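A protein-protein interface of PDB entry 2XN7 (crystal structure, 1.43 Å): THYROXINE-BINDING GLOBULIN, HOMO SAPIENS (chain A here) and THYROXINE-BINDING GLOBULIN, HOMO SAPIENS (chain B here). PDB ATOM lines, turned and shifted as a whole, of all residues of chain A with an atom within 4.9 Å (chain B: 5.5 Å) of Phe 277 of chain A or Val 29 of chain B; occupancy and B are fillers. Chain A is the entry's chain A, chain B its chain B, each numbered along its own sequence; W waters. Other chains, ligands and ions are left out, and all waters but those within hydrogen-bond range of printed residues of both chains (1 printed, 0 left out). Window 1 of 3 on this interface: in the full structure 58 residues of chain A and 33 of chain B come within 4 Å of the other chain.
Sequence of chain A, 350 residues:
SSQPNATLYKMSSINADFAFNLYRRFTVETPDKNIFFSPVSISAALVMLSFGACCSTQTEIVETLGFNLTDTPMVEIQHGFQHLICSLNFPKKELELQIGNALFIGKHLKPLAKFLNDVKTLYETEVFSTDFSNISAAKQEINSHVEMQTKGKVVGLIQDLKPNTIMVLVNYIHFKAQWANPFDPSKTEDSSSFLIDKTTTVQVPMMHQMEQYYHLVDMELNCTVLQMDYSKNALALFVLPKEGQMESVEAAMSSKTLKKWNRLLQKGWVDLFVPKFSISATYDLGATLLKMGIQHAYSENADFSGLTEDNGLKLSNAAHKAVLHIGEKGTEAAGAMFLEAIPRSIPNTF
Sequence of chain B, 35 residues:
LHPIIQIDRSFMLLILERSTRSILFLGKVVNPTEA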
ATOM      1  N   ASN A  34     -10.306 -30.825  -0.824  1.00  0.00           N
ATOM      2  CA  ASN A  34     -10.525 -29.787  -1.821  1.00  0.00           C
ATOM      3  C   ASN A  34     -11.126 -28.548  -1.186  1.00  0.00           C
ATOM      4  O   ASN A  34     -12.059 -28.641  -0.369  1.00  0.00           O
ATOM      5  CB  ASN A  34     -11.493 -30.259  -2.915  1.00  0.00           C
ATOM      6  CG  ASN A  34     -10.912 -31.353  -3.810  1.00  0.00           C
ATOM      7  OD1 ASN A  34      -9.697 -31.540  -3.895  1.00  0.00           O
ATOM      8  ND2 ASN A  34     -11.792 -32.060  -4.518  1.00  0.00           N
ATOM      9  N   PHE A 194      -2.816 -39.175 -10.516  1.00  0.00           N
ATOM     10  CA  PHE A 194      -2.757 -37.956  -9.714  1.00  0.00           C
ATOM     11  C   PHE A 194      -2.733 -38.415  -8.268  1.00  0.00           C
ATOM     12  O   PHE A 194      -3.627 -39.140  -7.839  1.00  0.00           O
ATOM     13  CB  PHE A 194      -3.972 -37.075  -9.973  1.00  0.00           C
ATOM     14  CG  PHE A 194      -3.907 -35.718  -9.308  1.00  0.00           C
ATOM     15  CD1 PHE A 194      -3.592 -34.586 -10.046  1.00  0.00           C
ATOM     16  CD2 PHE A 194      -4.174 -35.574  -7.961  1.00  0.00           C
ATOM     17  CE1 PHE A 194      -3.538 -33.336  -9.443  1.00  0.00           C
ATOM     18  CE2 PHE A 194      -4.112 -34.316  -7.350  1.00  0.00           C
ATOM     19  CZ  PHE A 194      -3.817 -33.211  -8.100  1.00  0.00           C
ATOM     20  N   PRO A 275      -4.070 -31.360 -15.257  1.00  0.00           N
ATOM     21  CA  PRO A 275      -5.223 -32.235 -15.308  1.00  0.00           C
ATOM     22  C   PRO A 275      -6.469 -31.542 -15.831  1.00  0.00           C
ATOM     23  O   PRO A 275      -6.643 -30.341 -15.638  1.00  0.00           O
ATOM     24  CB  PRO A 275      -5.411 -32.650 -13.848  1.00  0.00           C
ATOM     25  CG  PRO A 275      -4.852 -31.529 -13.060  1.00  0.00           C
ATOM     26  CD  PRO A 275      -3.701 -31.013 -13.881  1.00  0.00           C
ATOM     27  N   LYS A 276      -7.318 -32.321 -16.488  1.00  0.00           N
ATOM     28  CA  LYS A 276      -8.640 -31.903 -16.918  1.00  0.00           C
ATOM     29  C   LYS A 276      -9.610 -32.422 -15.890  1.00  0.00           C
ATOM     30  O   LYS A 276      -9.648 -33.632 -15.640  1.00  0.00           O
ATOM     31  CB  LYS A 276      -8.953 -32.511 -18.287  1.00  0.00           C
ATOM     32  CG  LYS A 276     -10.328 -32.269 -18.800  1.00  0.00           C
ATOM     33  CD  LYS A 276     -10.437 -32.720 -20.240  1.00  0.00           C
ATOM     34  CE  LYS A 276     -11.784 -32.418 -20.815  1.00  0.00           C
ATOM     35  NZ  LYS A 276     -11.841 -32.848 -22.228  1.00  0.00           N
ATOM     36  N   PHE A 277     -10.404 -31.539 -15.296  1.00  0.00           N
ATOM     37  CA  PHE A 277     -11.213 -31.925 -14.142  1.00  0.00           C
ATOM     38  C   PHE A 277     -12.235 -30.866 -13.777  1.00  0.00           C
ATOM     39  O   PHE A 277     -12.147 -29.726 -14.227  1.00  0.00           O
ATOM     40  CB  PHE A 277     -10.305 -32.176 -12.922  1.00  0.00           C
ATOM     41  CG  PHE A 277      -9.724 -30.918 -12.326  1.00  0.00           C
ATOM     42  CD1 PHE A 277     -10.252 -30.373 -11.164  1.00  0.00           C
ATOM     43  CD2 PHE A 277      -8.655 -30.258 -12.929  1.00  0.00           C
ATOM     44  CE1 PHE A 277      -9.732 -29.215 -10.618  1.00  0.00           C
ATOM     45  CE2 PHE A 277      -8.132 -29.090 -12.378  1.00  0.00           C
ATOM     46  CZ  PHE A 277      -8.691 -28.563 -11.218  1.00  0.00           C
ATOM     47  N   SER A 278     -13.184 -31.272 -12.935  1.00  0.00           N
ATOM     48  CA  SER A 278     -14.171 -30.373 -12.344  1.00  0.00           C
ATOM     49  C   SER A 278     -14.239 -30.642 -10.855  1.00  0.00           C
ATOM     50  O   SER A 278     -14.098 -31.788 -10.417  1.00  0.00           O
ATOM     51  CB  SER A 278     -15.562 -30.587 -12.933  1.00  0.00           C
ATOM     52  OG  SER A 278     -15.555 -30.515 -14.343  1.00  0.00           O
ATOM     53  N   ILE A 279     -14.485 -29.599 -10.079  1.00  0.00           N
ATOM     54  CA  ILE A 279     -14.825 -29.798  -8.678  1.00  0.00           C
ATOM     55  C   ILE A 279     -15.857 -28.770  -8.256  1.00  0.00           C
ATOM     56  O   ILE A 279     -16.128 -27.795  -8.960  1.00  0.00           O
ATOM     57  CB  ILE A 279     -13.602 -29.743  -7.740  1.00  0.00           C
ATOM     58  CG1 ILE A 279     -12.890 -28.399  -7.854  1.00  0.00           C
ATOM     59  CG2 ILE A 279     -12.635 -30.904  -8.024  1.00  0.00           C
ATOM     60  CD1 ILE A 279     -11.899 -28.104  -6.720  1.00  0.00           C
ATOM     61  N   LEU A 324     -15.851 -25.280 -10.473  1.00  0.00           N
ATOM     62  CA  LEU A 324     -14.713 -25.099 -11.362  1.00  0.00           C
ATOM     63  C   LEU A 324     -14.635 -26.213 -12.380  1.00  0.00           C
ATOM     64  O   LEU A 324     -14.765 -27.378 -12.024  1.00  0.00           O
ATOM     65  CB  LEU A 324     -13.430 -25.178 -10.540  1.00  0.00           C
ATOM     66  CG  LEU A 324     -12.081 -25.160 -11.278  1.00  0.00           C
ATOM     67  CD1 LEU A 324     -11.906 -23.833 -11.978  1.00  0.00           C
ATOM     68  CD2 LEU A 324     -10.928 -25.446 -10.320  1.00  0.00           C
ATOM     69  N   HIS A 325     -14.372 -25.846 -13.628  1.00  0.00           N
ATOM     70  CA  HIS A 325     -13.990 -26.810 -14.660  1.00  0.00           C
ATOM     71  C   HIS A 325     -12.776 -26.285 -15.410  1.00  0.00           C
ATOM     72  O   HIS A 325     -12.771 -25.130 -15.859  1.00  0.00           O
ATOM     73  CB  HIS A 325     -15.102 -27.084 -15.659  1.00  0.00           C
ATOM     74  CG  HIS A 325     -14.648 -27.923 -16.808  1.00  0.00           C
ATOM     75  ND1 HIS A 325     -14.425 -29.278 -16.694  1.00  0.00           N
ATOM     76  CD2 HIS A 325     -14.281 -27.585 -18.065  1.00  0.00           C
ATOM     77  CE1 HIS A 325     -13.993 -29.749 -17.852  1.00  0.00           C
ATOM     78  NE2 HIS A 325     -13.892 -28.741 -18.698  1.00  0.00           N
ATOM     79  N   ILE A 326     -11.767 -27.136 -15.558  1.00  0.00           N
ATOM     80  CA  ILE A 326     -10.580 -26.830 -16.348  1.00  0.00           C
ATOM     81  C   ILE A 326     -10.432 -27.920 -17.399  1.00  0.00           C
ATOM     82  O   ILE A 326     -10.508 -29.117 -17.089  1.00  0.00           O
ATOM     83  CB  ILE A 326      -9.323 -26.775 -15.468  1.00  0.00           C
ATOM     84  CG1 ILE A 326      -9.354 -25.486 -14.643  1.00  0.00           C
ATOM     85  CG2 ILE A 326      -8.051 -26.916 -16.325  1.00  0.00           C
ATOM     86  CD1 ILE A 326      -8.236 -25.366 -13.665  1.00  0.00           C
ATOM     87  N   ARG B   9      -0.180 -33.829  -8.385  1.00  0.00           N
ATOM     88  CA  ARG B   9      -0.398 -33.970  -6.950  1.00  0.00           C
ATOM     89  C   ARG B   9      -0.977 -32.650  -6.456  1.00  0.00           C
ATOM     90  O   ARG B   9      -1.105 -31.704  -7.239  1.00  0.00           O
ATOM     91  CB  ARG B   9       0.899 -34.311  -6.203  1.00  0.00           C
ATOM     92  CG  ARG B   9       2.011 -33.290  -6.382  1.00  0.00           C
ATOM     93  CD  ARG B   9       3.188 -33.541  -5.423  1.00  0.00           C
ATOM     94  NE  ARG B   9       4.173 -32.455  -5.479  1.00  0.00           N
ATOM     95  CZ  ARG B   9       5.060 -32.298  -6.458  1.00  0.00           C
ATOM     96  NH1 ARG B   9       5.110 -33.149  -7.475  1.00  0.00           N
ATOM     97  NH2 ARG B   9       5.910 -31.281  -6.428  1.00  0.00           N
ATOM     98  N   SER B  10      -1.303 -32.583  -5.174  1.00  0.00           N
ATOM     99  CA  SER B  10      -2.031 -31.438  -4.611  1.00  0.00           C
ATOM    100  C   SER B  10      -1.404 -30.092  -4.971  1.00  0.00           C
ATOM    101  O   SER B  10      -0.186 -29.912  -4.891  1.00  0.00           O
ATOM    102  CB  SER B  10      -2.100 -31.553  -3.096  1.00  0.00           C
ATOM    103  OG  SER B  10      -2.908 -32.640  -2.681  1.00  0.00           O
ATOM    104  N   PHE B  11      -2.249 -29.147  -5.363  1.00  0.00           N
ATOM    105  CA  PHE B  11      -1.800 -27.830  -5.765  1.00  0.00           C
ATOM    106  C   PHE B  11      -2.832 -26.791  -5.358  1.00  0.00           C
ATOM    107  O   PHE B  11      -4.020 -27.110  -5.211  1.00  0.00           O
ATOM    108  CB  PHE B  11      -1.549 -27.763  -7.278  1.00  0.00           C
ATOM    109  CG  PHE B  11      -2.767 -28.006  -8.143  1.00  0.00           C
ATOM    110  CD1 PHE B  11      -3.151 -29.292  -8.462  1.00  0.00           C
ATOM    111  CD2 PHE B  11      -3.502 -26.951  -8.655  1.00  0.00           C
ATOM    112  CE1 PHE B  11      -4.254 -29.520  -9.303  1.00  0.00           C
ATOM    113  CE2 PHE B  11      -4.598 -27.171  -9.492  1.00  0.00           C
ATOM    114  CZ  PHE B  11      -4.978 -28.452  -9.804  1.00  0.00           C
ATOM    115  N   MET B  12      -2.395 -25.546  -5.246  1.00  0.00           N
ATOM    116  CA  MET B  12      -3.296 -24.407  -5.058  1.00  0.00           C
ATOM    117  C   MET B  12      -3.490 -23.727  -6.410  1.00  0.00           C
ATOM    118  O   MET B  12      -2.627 -23.773  -7.302  1.00  0.00           O
ATOM    119  CB  MET B  12      -2.755 -23.425  -4.009  1.00  0.00           C
ATOM    120  CG  MET B  12      -2.990 -23.840  -2.560  1.00  0.00           C
ATOM    121  SD  MET B  12      -2.364 -22.638  -1.364  1.00  0.00           S
ATOM    122  CE  MET B  12      -3.633 -21.377  -1.476  1.00  0.00           C
ATOM    123  N   LEU B  13      -4.653 -23.105  -6.549  1.00  0.00           N
ATOM    124  CA  LEU B  13      -5.041 -22.437  -7.770  1.00  0.00           C
ATOM    125  C   LEU B  13      -5.632 -21.079  -7.441  1.00  0.00           C
ATOM    126  O   LEU B  13      -6.483 -20.980  -6.558  1.00  0.00           O
ATOM    127  CB  LEU B  13      -6.096 -23.264  -8.502  1.00  0.00           C
ATOM    128  CG  LEU B  13      -6.748 -22.669  -9.748  1.00  0.00           C
ATOM    129  CD1 LEU B  13      -5.726 -22.505 -10.892  1.00  0.00           C
ATOM    130  CD2 LEU B  13      -7.928 -23.537 -10.228  1.00  0.00           C
ATOM    131  N   GLY B  27      -8.436 -21.784  -4.620  1.00  0.00           N
ATOM    132  CA  GLY B  27      -8.684 -23.129  -4.184  1.00  0.00           C
ATOM    133  C   GLY B  27      -7.456 -23.971  -3.990  1.00  0.00           C
ATOM    134  O   GLY B  27      -6.339 -23.552  -4.256  1.00  0.00           O
ATOM    135  N   LYS B  28      -7.715 -25.174  -3.509  1.00  0.00           N
ATOM    136  CA  LYS B  28      -6.724 -26.233  -3.418  1.00  0.00           C
ATOM    137  C   LYS B  28      -7.367 -27.496  -3.956  1.00  0.00           C
ATOM    138  O   LYS B  28      -8.463 -27.862  -3.538  1.00  0.00           O
ATOM    139  CB  LYS B  28      -6.277 -26.462  -1.989  1.00  0.00           C
ATOM    140  CG  LYS B  28      -5.367 -27.678  -1.839  1.00  0.00           C
ATOM    141  CD  LYS B  28      -4.773 -27.823  -0.469  1.00  0.00           C
ATOM    142  CE  LYS B  28      -5.826 -27.962   0.623  1.00  0.00           C
ATOM    143  NZ  LYS B  28      -5.228 -28.166   1.994  1.00  0.00           N
ATOM    144  N   VAL B  29      -6.674 -28.145  -4.873  1.00  0.00           N
ATOM    145  CA  VAL B  29      -7.149 -29.376  -5.495  1.00  0.00           C
ATOM    146  C   VAL B  29      -6.308 -30.498  -4.895  1.00  0.00           C
ATOM    147  O   VAL B  29      -5.093 -30.581  -5.139  1.00  0.00           O
ATOM    148  CB  VAL B  29      -7.026 -29.331  -7.031  1.00  0.00           C
ATOM    149  CG1 VAL B  29      -7.475 -30.657  -7.656  1.00  0.00           C
ATOM    150  CG2 VAL B  29      -7.851 -28.163  -7.606  1.00  0.00           C
ATOM    151  N   VAL B  30      -6.968 -31.317  -4.080  1.00  0.00           N
ATOM    152  CA  VAL B  30      -6.368 -32.502  -3.458  1.00  0.00           C
ATOM    153  C   VAL B  30      -6.782 -33.759  -4.217  1.00  0.00           C
ATOM    154  O   VAL B  30      -5.954 -34.630  -4.486  1.00  0.00           O
ATOM    155  CB  VAL B  30      -6.804 -32.625  -1.984  1.00  0.00           C
ATOM    156  CG1 VAL B  30      -6.341 -33.959  -1.405  1.00  0.00           C
ATOM    157  CG2 VAL B  30      -6.256 -31.450  -1.168  1.00  0.00           C
ATOM    158  N   ASN B  31      -8.066 -33.845  -4.561  1.00  0.00           N
ATOM    159  CA  ASN B  31      -8.601 -34.956  -5.339  1.00  0.00           C
ATOM    160  C   ASN B  31      -9.458 -34.416  -6.472  1.00  0.00           C
ATOM    161  O   ASN B  31     -10.627 -34.056  -6.261  1.00  0.00           O
ATOM    162  CB  ASN B  31      -9.406 -35.919  -4.459  1.00  0.00           C
ATOM    163  CG  ASN B  31      -9.953 -37.104  -5.237  1.00  0.00           C
ATOM    164  OD1 ASN B  31      -9.779 -37.191  -6.446  1.00  0.00           O
ATOM    165  ND2 ASN B  31     -10.621 -38.019  -4.542  1.00  0.00           N
ATOM    166  N   PRO B  32      -8.891 -34.363  -7.681  1.00  0.00           N
ATOM    167  CA  PRO B  32      -9.620 -33.775  -8.796  1.00  0.00           C
ATOM    168  C   PRO B  32     -10.818 -34.585  -9.292  1.00  0.00           C
ATOM    169  O   PRO B  32     -11.547 -34.091 -10.139  1.00  0.00           O
ATOM    170  CB  PRO B  32      -8.554 -33.647  -9.887  1.00  0.00           C
ATOM    171  CG  PRO B  32      -7.533 -34.649  -9.543  1.00  0.00           C
ATOM    172  CD  PRO B  32      -7.541 -34.806  -8.068  1.00  0.00           C
HETATM  173  O   HOH W   1     -13.031 -34.274 -12.458  1.00  0.00           O
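The side-chain amide oxygen of Asn 34 of chain A is in hydrogen-bond range of the backbone NH of Val 30 of chain B (2.7 Å). O of Asn 31 of chain B lies within hydrogen-bond range of ND2 of Asn 34 of chain A (2.9 Å). The backbone carbonyl oxygen of Ser 278 of chain A sits close to the backbone carbonyl oxygen of Pro 32 of chain B (3.4 Å).
A ring nitrogen (ND1) of His 325 of chain A sits at hydrogen-bond distance from the backbone carbonyl oxygen (O) of Phe 277 of chain A (3.4 Å). The backbone NH (N) of Ile 326 of chain A lies within hydrogen-bond range of the backbone carbonyl oxygen (O) of Phe 277 of chain A (2.9 Å). The side-chain hydroxyl of Ser 278 of chain A is in hydrogen-bond range of a ring nitrogen (ND1) of His 325 of chain A, 2.9 Å away. The backbone NH (N) of Leu 324 of chain A sits at hydrogen-bond distance from the backbone carbonyl oxygen (O) of Ile 279 of chain A (2.9 Å). The backbone NH (N) of Val 29 of chain B sits at hydrogen-bond distance from the backbone carbonyl oxygen (O) of Phe 11 of chain B (2.9 Å). The backbone NH of Gly 27 of chain B is in hydrogen-bond range of the backbone carbonyl oxygen of Leu 13 of chain B.
Val 29 of chain B touches Asn 34 of chain A. CZ of Phe 194 of chain A touches O of Arg 9 of chain B, 3.2 Å away. Phe 194 of chain A touches Phe 11 of chain B. Pro 32 of chain B touches Phe 194 of chain A. CZ of Phe 11 of chain B touches CZ of Phe 277 of chain A (3.97 Å). CG2 of Val 29 of chain B touches CE1 of Phe 277 of chain A, at 3.7 Å. Phe 277 of chain A touches Pro 32 of chain B (CB to O, 3.6 Å). Ile 279 of chain A touches Pro 32 of chain B (CG2 to O, 3.98 Å). CD2 of Leu 324 of chain A touches CD2 of Leu 13 of chain B, at 3.6 Å. CD2 of Leu 13 of chain B touches CD1 of Ile 326 of chain A, at 3.9 Å.
Phe 277 of chain A touches just these residues of chain B: Phe 11, Val 29 and Pro 32. Of chain A, only Asn 34 (3.7 Å) and Phe 277 (3.7 Å) come within 4 Å of Val 29 of chain B. Printed residues of chain A within 4 Å of Asn 31 of chain B: Asn 34. Of the printed residues of chain B, Phe 194 of chain A touches Arg 9, Ser 10, Phe 11, Val 30 and Pro 32. Of the printed residues of chain B, Ile 326 of chain A touches Leu 13 (3.9 Å). The nearest residue of chain B that does not touch Phe 277 of chain A is Leu 13 of chain B (5.2 Å). The nearest printed residue of chain B that does not touch Asn 34 of chain A is Pro 32 of chain B (4.8 Å).
Of the 11 printed residues of chain B, 9 touch a printed residue of chain A. Printed residues of chain B that touch a printed residue of chain A: Arg 9, Ser 10, Phe 11, Leu 13, Lys 28, Val 29, Val 30, Asn 31 and Pro 32. Hydrophobic or aromatic side chains of chain B within 4 Å of the printed part of chain A: Phe 11, Leu 13, Val 29, Val 30 and Pro 32. Of the 10 printed residues of chain A, 7 touch a printed residue of chain B. Hydrophobic or aromatic side chains of chain A that line the printed part of chain B: Phe 194, Phe 277, Ile 279, Leu 324 and Ile 326. Among the printed residues, 16 pairs touch across the chains. Among the printed residues, no Asp or Glu carboxylate lies within 4 Å of a Lys or Arg side-chain nitrogen of the other chain.
Water W1 bridges O of Pro 32 of chain B (2.8 Å) and N of Ser 278 of chain A (3.0 Å).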
